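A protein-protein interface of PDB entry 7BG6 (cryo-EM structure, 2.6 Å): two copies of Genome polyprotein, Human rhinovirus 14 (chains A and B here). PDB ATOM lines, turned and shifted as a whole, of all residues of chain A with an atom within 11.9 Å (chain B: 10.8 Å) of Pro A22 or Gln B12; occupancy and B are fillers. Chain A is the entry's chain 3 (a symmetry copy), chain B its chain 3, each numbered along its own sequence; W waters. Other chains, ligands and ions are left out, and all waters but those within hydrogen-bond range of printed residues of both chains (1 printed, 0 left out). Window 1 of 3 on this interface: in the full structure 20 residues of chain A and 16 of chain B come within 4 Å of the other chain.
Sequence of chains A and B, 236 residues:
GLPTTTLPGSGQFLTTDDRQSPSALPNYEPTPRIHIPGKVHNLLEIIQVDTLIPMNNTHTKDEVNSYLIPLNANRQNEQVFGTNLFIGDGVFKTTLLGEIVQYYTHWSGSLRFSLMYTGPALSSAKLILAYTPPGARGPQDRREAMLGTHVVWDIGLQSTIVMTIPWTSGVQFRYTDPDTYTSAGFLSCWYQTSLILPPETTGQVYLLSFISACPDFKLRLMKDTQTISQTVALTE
The side-chain hydroxyl of Thr B16 sits close to the backbone carbonyl oxygen of Ala A24 (3.4 Å).
The backbone NH (N) of Gly A11 is in hydrogen-bond range of the backbone carbonyl oxygen (O) of Thr B6, at 2.7 Å.
OG of Ser A23 sits close to N of Leu A25, at 3.3 Å.
OD1 of Asp B17 lies within salt-bridge range of NH1 of Arg B19, at 3.9 Å.
O of Leu B7 is in hydrogen-bond range of OG of Ser B10 (2.9 Å).
Among the printed residues, pairs that only touch across the chains: Gln A12 with Pro B8 (3.2 Å), Pro A22 with Asp B17 (3.3 Å), Pro A22 with Gln B12 (3.6 Å), Arg A19 with Leu B7 (3.6 Å), Pro A26 with Thr B16 (3.7 Å), Pro A22 with Leu B14 (3.7 Å) and Ser A23 with Thr B16 (3.8 Å).
Pro A22 touches three residues of chain B.
No residue of chain B comes within 4 Å of Ser A21.
Printed residues of chain B within 4 Å of Ser A23: Thr B16.
Leu B14 touches one residue of chain A.
Of chain A, only Pro A22 comes within 4 Å of Asp B17.
Printed residues of chain A within 4 Å of Leu B7: Arg A19 (3.6 Å).
Printed residues of chain B within 4 Å of Arg A19: Leu B7.
Of the printed residues of chain B, Ala A24 touches Thr B16.
The nearest residue of chain B that does not touch Pro A22 is Arg B19 (6.1 Å).
The nearest residue of chain A that does not touch Gln B12 is Ser A21 (6.7 Å).
Of the 14 printed residues of chain B, 7 touch a printed residue of chain A.
Of the 14 printed residues of chain A, 7 touch a printed residue of chain B.
Hydrophobic or aromatic side chains of chain A within 4 Å of the printed part of chain B: Pro A22 and Pro A26.
Among the printed residues, no Asp or Glu carboxylate lies within 4 Å of a Lys or Arg side-chain nitrogen of the other chain.
Positions printed for both chains: 11, 12, 13, 18 and 19.
Of the 9 pairs that touch across the chains among the printed residues, none has its exchanged pair printed and touching as well.
Water W1 bridges O of Gln A12 and O of Thr B6.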
ATOM      1  N   GLY A  11     -27.639 -13.991   2.647  1.00  0.00           N
ATOM      2  CA  GLY A  11     -27.663 -13.053   1.538  1.00  0.00           C
ATOM      3  C   GLY A  11     -28.925 -12.193   1.547  1.00  0.00           C
ATOM      4  O   GLY A  11     -29.206 -11.492   0.577  1.00  0.00           O
ATOM      5  N   GLN A  12     -29.677 -12.264   2.654  1.00  0.00           N
ATOM      6  CA  GLN A  12     -30.872 -11.456   2.834  1.00  0.00           C
ATOM      7  C   GLN A  12     -30.470 -10.079   3.351  1.00  0.00           C
ATOM      8  O   GLN A  12     -29.523  -9.953   4.126  1.00  0.00           O
ATOM      9  CB  GLN A  12     -31.857 -12.144   3.786  1.00  0.00           C
ATOM     10  CG  GLN A  12     -31.494 -12.008   5.261  1.00  0.00           C
ATOM     11  CD  GLN A  12     -32.493 -12.635   6.204  1.00  0.00           C
ATOM     12  OE1 GLN A  12     -33.583 -13.044   5.812  1.00  0.00           O
ATOM     13  NE2 GLN A  12     -32.125 -12.709   7.472  1.00  0.00           N
ATOM     14  N   PHE A  13     -31.196  -9.050   2.900  1.00  0.00           N
ATOM     15  CA  PHE A  13     -31.035  -7.710   3.444  1.00  0.00           C
ATOM     16  C   PHE A  13     -32.208  -7.402   4.370  1.00  0.00           C
ATOM     17  O   PHE A  13     -33.327  -7.179   3.913  1.00  0.00           O
ATOM     18  CB  PHE A  13     -30.842  -6.672   2.333  1.00  0.00           C
ATOM     19  CG  PHE A  13     -30.931  -5.235   2.784  1.00  0.00           C
ATOM     20  CD1 PHE A  13     -30.324  -4.813   3.960  1.00  0.00           C
ATOM     21  CD2 PHE A  13     -31.611  -4.294   2.023  1.00  0.00           C
ATOM     22  CE1 PHE A  13     -30.412  -3.492   4.373  1.00  0.00           C
ATOM     23  CE2 PHE A  13     -31.694  -2.972   2.435  1.00  0.00           C
ATOM     24  CZ  PHE A  13     -31.094  -2.573   3.609  1.00  0.00           C
ATOM     25  N   ASP A  18     -28.326  -5.199  13.000  1.00  0.00           N
ATOM     26  CA  ASP A  18     -27.234  -4.312  13.366  1.00  0.00           C
ATOM     27  C   ASP A  18     -25.918  -5.083  13.305  1.00  0.00           C
ATOM     28  O   ASP A  18     -25.435  -5.585  14.318  1.00  0.00           O
ATOM     29  CB  ASP A  18     -27.500  -3.660  14.729  1.00  0.00           C
ATOM     30  CG  ASP A  18     -26.366  -2.790  15.247  1.00  0.00           C
ATOM     31  OD1 ASP A  18     -26.121  -2.823  16.470  1.00  0.00           O
ATOM     32  OD2 ASP A  18     -25.742  -2.082  14.431  1.00  0.00           O
ATOM     33  N   ARG A  19     -25.349  -5.165  12.096  1.00  0.00           N
ATOM     34  CA  ARG A  19     -24.126  -5.917  11.863  1.00  0.00           C
ATOM     35  C   ARG A  19     -22.966  -4.957  11.618  1.00  0.00           C
ATOM     36  O   ARG A  19     -23.173  -3.802  11.250  1.00  0.00           O
ATOM     37  CB  ARG A  19     -24.275  -6.854  10.660  1.00  0.00           C
ATOM     38  CG  ARG A  19     -25.438  -7.834  10.738  1.00  0.00           C
ATOM     39  CD  ARG A  19     -25.640  -8.516  12.080  1.00  0.00           C
ATOM     40  NE  ARG A  19     -24.467  -9.147  12.664  1.00  0.00           N
ATOM     41  CZ  ARG A  19     -24.350  -9.469  13.946  1.00  0.00           C
ATOM     42  NH1 ARG A  19     -25.336  -9.217  14.791  1.00  0.00           N
ATOM     43  NH2 ARG A  19     -23.242 -10.040  14.385  1.00  0.00           N
ATOM     44  N   GLN A  20     -21.747  -5.468  11.826  1.00  0.00           N
ATOM     45  CA  GLN A  20     -20.527  -4.775  11.445  1.00  0.00           C
ATOM     46  C   GLN A  20     -20.433  -4.751   9.923  1.00  0.00           C
ATOM     47  O   GLN A  20     -21.015  -5.601   9.249  1.00  0.00           O
ATOM     48  CB  GLN A  20     -19.302  -5.471  12.040  1.00  0.00           C
ATOM     49  CG  GLN A  20     -19.262  -5.472  13.563  1.00  0.00           C
ATOM     50  CD  GLN A  20     -18.023  -6.146  14.101  1.00  0.00           C
ATOM     51  OE1 GLN A  20     -16.907  -5.894  13.651  1.00  0.00           O
ATOM     52  NE2 GLN A  20     -18.212  -7.013  15.082  1.00  0.00           N
ATOM     53  N   SER A  21     -19.692  -3.771   9.395  1.00  0.00           N
ATOM     54  CA  SER A  21     -19.516  -3.604   7.962  1.00  0.00           C
ATOM     55  C   SER A  21     -18.175  -2.928   7.684  1.00  0.00           C
ATOM     56  O   SER A  21     -17.663  -2.206   8.537  1.00  0.00           O
ATOM     57  CB  SER A  21     -20.661  -2.824   7.366  1.00  0.00           C
ATOM     58  OG  SER A  21     -20.806  -1.566   8.007  1.00  0.00           O
ATOM     59  N   PRO A  22     -17.560  -3.140   6.496  1.00  0.00           N
ATOM     60  CA  PRO A  22     -16.301  -2.474   6.156  1.00  0.00           C
ATOM     61  C   PRO A  22     -16.490  -0.977   5.928  1.00  0.00           C
ATOM     62  O   PRO A  22     -17.427  -0.562   5.246  1.00  0.00           O
ATOM     63  CB  PRO A  22     -15.860  -3.174   4.861  1.00  0.00           C
ATOM     64  CG  PRO A  22     -17.150  -3.680   4.249  1.00  0.00           C
ATOM     65  CD  PRO A  22     -18.029  -4.039   5.429  1.00  0.00           C
ATOM     66  N   SER A  23     -15.595  -0.178   6.517  1.00  0.00           N
ATOM     67  CA  SER A  23     -15.623   1.265   6.351  1.00  0.00           C
ATOM     68  C   SER A  23     -15.027   1.641   4.997  1.00  0.00           C
ATOM     69  O   SER A  23     -13.988   1.113   4.601  1.00  0.00           O
ATOM     70  CB  SER A  23     -14.920   1.961   7.485  1.00  0.00           C
ATOM     71  OG  SER A  23     -14.796   3.354   7.232  1.00  0.00           O
ATOM     72  N   ALA A  24     -15.705   2.563   4.302  1.00  0.00           N
ATOM     73  CA  ALA A  24     -15.315   2.996   2.970  1.00  0.00           C
ATOM     74  C   ALA A  24     -14.304   4.137   3.060  1.00  0.00           C
ATOM     75  O   ALA A  24     -13.732   4.541   2.050  1.00  0.00           O
ATOM     76  CB  ALA A  24     -16.538   3.398   2.185  1.00  0.00           C
ATOM     77  N   LEU A  25     -14.101   4.655   4.277  1.00  0.00           N
ATOM     78  CA  LEU A  25     -13.111   5.690   4.527  1.00  0.00           C
ATOM     79  C   LEU A  25     -12.185   5.231   5.651  1.00  0.00           C
ATOM     80  O   LEU A  25     -12.384   5.598   6.808  1.00  0.00           O
ATOM     81  CB  LEU A  25     -13.824   6.998   4.888  1.00  0.00           C
ATOM     82  CG  LEU A  25     -14.753   7.579   3.821  1.00  0.00           C
ATOM     83  CD1 LEU A  25     -15.547   8.746   4.381  1.00  0.00           C
ATOM     84  CD2 LEU A  25     -13.973   8.015   2.591  1.00  0.00           C
ATOM     85  N   PRO A  26     -11.152   4.408   5.351  1.00  0.00           N
ATOM     86  CA  PRO A  26     -10.248   3.900   6.384  1.00  0.00           C
ATOM     87  C   PRO A  26      -9.293   4.978   6.892  1.00  0.00           C
ATOM     88  O   PRO A  26      -8.823   5.811   6.119  1.00  0.00           O
ATOM     89  CB  PRO A  26      -9.475   2.783   5.666  1.00  0.00           C
ATOM     90  CG  PRO A  26      -9.486   3.193   4.207  1.00  0.00           C
ATOM     91  CD  PRO A  26     -10.799   3.923   4.005  1.00  0.00           C
ATOM     92  N   ASN A  27      -9.043   4.952   8.208  1.00  0.00           N
ATOM     93  CA  ASN A  27      -8.092   5.827   8.877  1.00  0.00           C
ATOM     94  C   ASN A  27      -8.582   7.274   8.857  1.00  0.00           C
ATOM     95  O   ASN A  27      -7.833   8.187   9.195  1.00  0.00           O
ATOM     96  CB  ASN A  27      -6.673   5.685   8.312  1.00  0.00           C
ATOM     97  CG  ASN A  27      -6.166   4.258   8.319  1.00  0.00           C
ATOM     98  OD1 ASN A  27      -6.088   3.623   9.369  1.00  0.00           O
ATOM     99  ND2 ASN A  27      -5.808   3.747   7.152  1.00  0.00           N
ATOM    100  N   TYR A  28      -9.845   7.473   8.459  1.00  0.00           N
ATOM    101  CA  TYR A  28     -10.447   8.795   8.457  1.00  0.00           C
ATOM    102  C   TYR A  28     -10.753   9.210   9.894  1.00  0.00           C
ATOM    103  O   TYR A  28     -11.325   8.434  10.659  1.00  0.00           O
ATOM    104  CB  TYR A  28     -11.700   8.827   7.576  1.00  0.00           C
ATOM    105  CG  TYR A  28     -12.519  10.091   7.684  1.00  0.00           C
ATOM    106  CD1 TYR A  28     -12.347  11.136   6.789  1.00  0.00           C
ATOM    107  CD2 TYR A  28     -13.464  10.246   8.686  1.00  0.00           C
ATOM    108  CE1 TYR A  28     -13.094  12.301   6.886  1.00  0.00           C
ATOM    109  CE2 TYR A  28     -14.220  11.403   8.796  1.00  0.00           C
ATOM    110  CZ  TYR A  28     -14.033  12.433   7.894  1.00  0.00           C
ATOM    111  OH  TYR A  28     -14.771  13.576   7.995  1.00  0.00           O
ATOM    112  N   THR B   6     -24.513 -15.642   5.637  1.00  0.00           N
ATOM    113  CA  THR B   6     -23.813 -14.626   4.867  1.00  0.00           C
ATOM    114  C   THR B   6     -24.610 -13.325   4.892  1.00  0.00           C
ATOM    115  O   THR B   6     -25.782 -13.300   4.519  1.00  0.00           O
ATOM    116  CB  THR B   6     -23.499 -15.105   3.441  1.00  0.00           C
ATOM    117  OG1 THR B   6     -24.726 -15.313   2.743  1.00  0.00           O
ATOM    118  CG2 THR B   6     -22.662 -16.365   3.405  1.00  0.00           C
ATOM    119  N   LEU B   7     -23.951 -12.253   5.345  1.00  0.00           N
ATOM    120  CA  LEU B   7     -24.549 -10.929   5.417  1.00  0.00           C
ATOM    121  C   LEU B   7     -24.678 -10.357   4.008  1.00  0.00           C
ATOM    122  O   LEU B   7     -24.014 -10.827   3.086  1.00  0.00           O
ATOM    123  CB  LEU B   7     -23.664 -10.027   6.285  1.00  0.00           C
ATOM    124  CG  LEU B   7     -23.531 -10.421   7.755  1.00  0.00           C
ATOM    125  CD1 LEU B   7     -22.683  -9.404   8.500  1.00  0.00           C
ATOM    126  CD2 LEU B   7     -24.896 -10.555   8.417  1.00  0.00           C
ATOM    127  N   PRO B   8     -25.538  -9.332   3.795  1.00  0.00           N
ATOM    128  CA  PRO B   8     -25.555  -8.597   2.530  1.00  0.00           C
ATOM    129  C   PRO B   8     -24.248  -7.826   2.365  1.00  0.00           C
ATOM    130  O   PRO B   8     -23.637  -7.416   3.351  1.00  0.00           O
ATOM    131  CB  PRO B   8     -26.748  -7.639   2.670  1.00  0.00           C
ATOM    132  CG  PRO B   8     -26.946  -7.497   4.163  1.00  0.00           C
ATOM    133  CD  PRO B   8     -26.539  -8.833   4.750  1.00  0.00           C
ATOM    134  N   GLY B   9     -23.830  -7.643   1.109  1.00  0.00           N
ATOM    135  CA  GLY B   9     -22.524  -7.082   0.810  1.00  0.00           C
ATOM    136  C   GLY B   9     -21.445  -8.162   0.801  1.00  0.00           C
ATOM    137  O   GLY B   9     -20.263  -7.866   0.957  1.00  0.00           O
ATOM    138  N   SER B  10     -21.882  -9.417   0.635  1.00  0.00           N
ATOM    139  CA  SER B  10     -20.984 -10.550   0.481  1.00  0.00           C
ATOM    140  C   SER B  10     -20.649 -10.733  -0.996  1.00  0.00           C
ATOM    141  O   SER B  10     -21.544 -10.787  -1.838  1.00  0.00           O
ATOM    142  CB  SER B  10     -21.583 -11.802   1.066  1.00  0.00           C
ATOM    143  OG  SER B  10     -21.388 -11.847   2.472  1.00  0.00           O
ATOM    144  N   GLY B  11     -19.347 -10.824  -1.290  1.00  0.00           N
ATOM    145  CA  GLY B  11     -18.864 -10.962  -2.654  1.00  0.00           C
ATOM    146  C   GLY B  11     -18.679  -9.606  -3.332  1.00  0.00           C
ATOM    147  O   GLY B  11     -18.473  -9.541  -4.542  1.00  0.00           O
ATOM    148  N   GLN B  12     -18.760  -8.534  -2.535  1.00  0.00           N
ATOM    149  CA  GLN B  12     -18.544  -7.182  -3.025  1.00  0.00           C
ATOM    150  C   GLN B  12     -17.045  -6.893  -3.044  1.00  0.00           C
ATOM    151  O   GLN B  12     -16.308  -7.356  -2.175  1.00  0.00           O
ATOM    152  CB  GLN B  12     -19.298  -6.162  -2.164  1.00  0.00           C
ATOM    153  CG  GLN B  12     -18.613  -5.835  -0.842  1.00  0.00           C
ATOM    154  CD  GLN B  12     -19.324  -4.788  -0.019  1.00  0.00           C
ATOM    155  OE1 GLN B  12     -20.259  -4.135  -0.474  1.00  0.00           O
ATOM    156  NE2 GLN B  12     -18.873  -4.613   1.211  1.00  0.00           N
ATOM    157  N   PHE B  13     -16.609  -6.133  -4.054  1.00  0.00           N
ATOM    158  CA  PHE B  13     -15.243  -5.637  -4.096  1.00  0.00           C
ATOM    159  C   PHE B  13     -15.235  -4.157  -3.724  1.00  0.00           C
ATOM    160  O   PHE B  13     -15.661  -3.311  -4.505  1.00  0.00           O
ATOM    161  CB  PHE B  13     -14.579  -5.933  -5.446  1.00  0.00           C
ATOM    162  CG  PHE B  13     -13.264  -5.229  -5.676  1.00  0.00           C
ATOM    163  CD1 PHE B  13     -12.311  -5.145  -4.669  1.00  0.00           C
ATOM    164  CD2 PHE B  13     -12.969  -4.660  -6.907  1.00  0.00           C
ATOM    165  CE1 PHE B  13     -11.105  -4.494  -4.883  1.00  0.00           C
ATOM    166  CE2 PHE B  13     -11.760  -4.014  -7.121  1.00  0.00           C
ATOM    167  CZ  PHE B  13     -10.830  -3.932  -6.109  1.00  0.00           C
ATOM    168  N   LEU B  14     -14.746  -3.876  -2.511  1.00  0.00           N
ATOM    169  CA  LEU B  14     -14.614  -2.522  -1.999  1.00  0.00           C
ATOM    170  C   LEU B  14     -13.138  -2.133  -2.019  1.00  0.00           C
ATOM    171  O   LEU B  14     -12.306  -2.812  -1.419  1.00  0.00           O
ATOM    172  CB  LEU B  14     -15.198  -2.478  -0.582  1.00  0.00           C
ATOM    173  CG  LEU B  14     -14.983  -1.182   0.200  1.00  0.00           C
ATOM    174  CD1 LEU B  14     -15.721  -0.018  -0.443  1.00  0.00           C
ATOM    175  CD2 LEU B  14     -15.417  -1.346   1.648  1.00  0.00           C
ATOM    176  N   THR B  15     -12.839  -1.024  -2.704  1.00  0.00           N
ATOM    177  CA  THR B  15     -11.475  -0.630  -3.026  1.00  0.00           C
ATOM    178  C   THR B  15     -10.733  -0.125  -1.787  1.00  0.00           C
ATOM    179  O   THR B  15      -9.545   0.180  -1.864  1.00  0.00           O
ATOM    180  CB  THR B  15     -11.450   0.415  -4.152  1.00  0.00           C
ATOM    181  OG1 THR B  15     -12.197   1.557  -3.732  1.00  0.00           O
ATOM    182  CG2 THR B  15     -12.001  -0.107  -5.461  1.00  0.00           C
ATOM    183  N   THR B  16     -11.434  -0.056  -0.647  1.00  0.00           N
ATOM    184  CA  THR B  16     -10.893   0.585   0.542  1.00  0.00           C
ATOM    185  C   THR B  16     -10.642  -0.422   1.663  1.00  0.00           C
ATOM    186  O   THR B  16      -9.910  -0.118   2.605  1.00  0.00           O
ATOM    187  CB  THR B  16     -11.781   1.745   1.015  1.00  0.00           C
ATOM    188  OG1 THR B  16     -13.149   1.342   0.942  1.00  0.00           O
ATOM    189  CG2 THR B  16     -11.580   3.007   0.208  1.00  0.00           C
ATOM    190  N   ASP B  17     -11.247  -1.610   1.558  1.00  0.00           N
ATOM    191  CA  ASP B  17     -11.192  -2.592   2.630  1.00  0.00           C
ATOM    192  C   ASP B  17      -9.814  -3.248   2.673  1.00  0.00           C
ATOM    193  O   ASP B  17      -9.289  -3.677   1.646  1.00  0.00           O
ATOM    194  CB  ASP B  17     -12.332  -3.611   2.524  1.00  0.00           C
ATOM    195  CG  ASP B  17     -12.550  -4.414   3.794  1.00  0.00           C
ATOM    196  OD1 ASP B  17     -11.772  -4.226   4.755  1.00  0.00           O
ATOM    197  OD2 ASP B  17     -13.496  -5.226   3.813  1.00  0.00           O
ATOM    198  N   ASP B  18      -9.251  -3.325   3.886  1.00  0.00           N
ATOM    199  CA  ASP B  18      -7.912  -3.841   4.118  1.00  0.00           C
ATOM    200  C   ASP B  18      -8.012  -5.238   4.728  1.00  0.00           C
ATOM    201  O   ASP B  18      -7.948  -5.398   5.947  1.00  0.00           O
ATOM    202  CB  ASP B  18      -7.092  -2.860   4.964  1.00  0.00           C
ATOM    203  CG  ASP B  18      -5.707  -3.357   5.349  1.00  0.00           C
ATOM    204  OD1 ASP B  18      -5.289  -3.083   6.492  1.00  0.00           O
ATOM    205  OD2 ASP B  18      -5.056  -4.006   4.505  1.00  0.00           O
ATOM    206  N   ARG B  19      -8.169  -6.242   3.858  1.00  0.00           N
ATOM    207  CA  ARG B  19      -8.341  -7.620   4.287  1.00  0.00           C
ATOM    208  C   ARG B  19      -7.081  -8.422   3.975  1.00  0.00           C
ATOM    209  O   ARG B  19      -6.287  -8.036   3.119  1.00  0.00           O
ATOM    210  CB  ARG B  19      -9.543  -8.269   3.591  1.00  0.00           C
ATOM    211  CG  ARG B  19     -10.868  -7.540   3.764  1.00  0.00           C
ATOM    212  CD  ARG B  19     -11.166  -7.033   5.165  1.00  0.00           C
ATOM    213  NE  ARG B  19     -11.029  -8.003   6.241  1.00  0.00           N
ATOM    214  CZ  ARG B  19     -10.896  -7.683   7.523  1.00  0.00           C
ATOM    215  NH1 ARG B  19     -10.877  -6.415   7.897  1.00  0.00           N
ATOM    216  NH2 ARG B  19     -10.778  -8.635   8.431  1.00  0.00           N
HETATM  217  O   HOH W   1     -27.838 -11.502   6.462  1.00  0.00           O
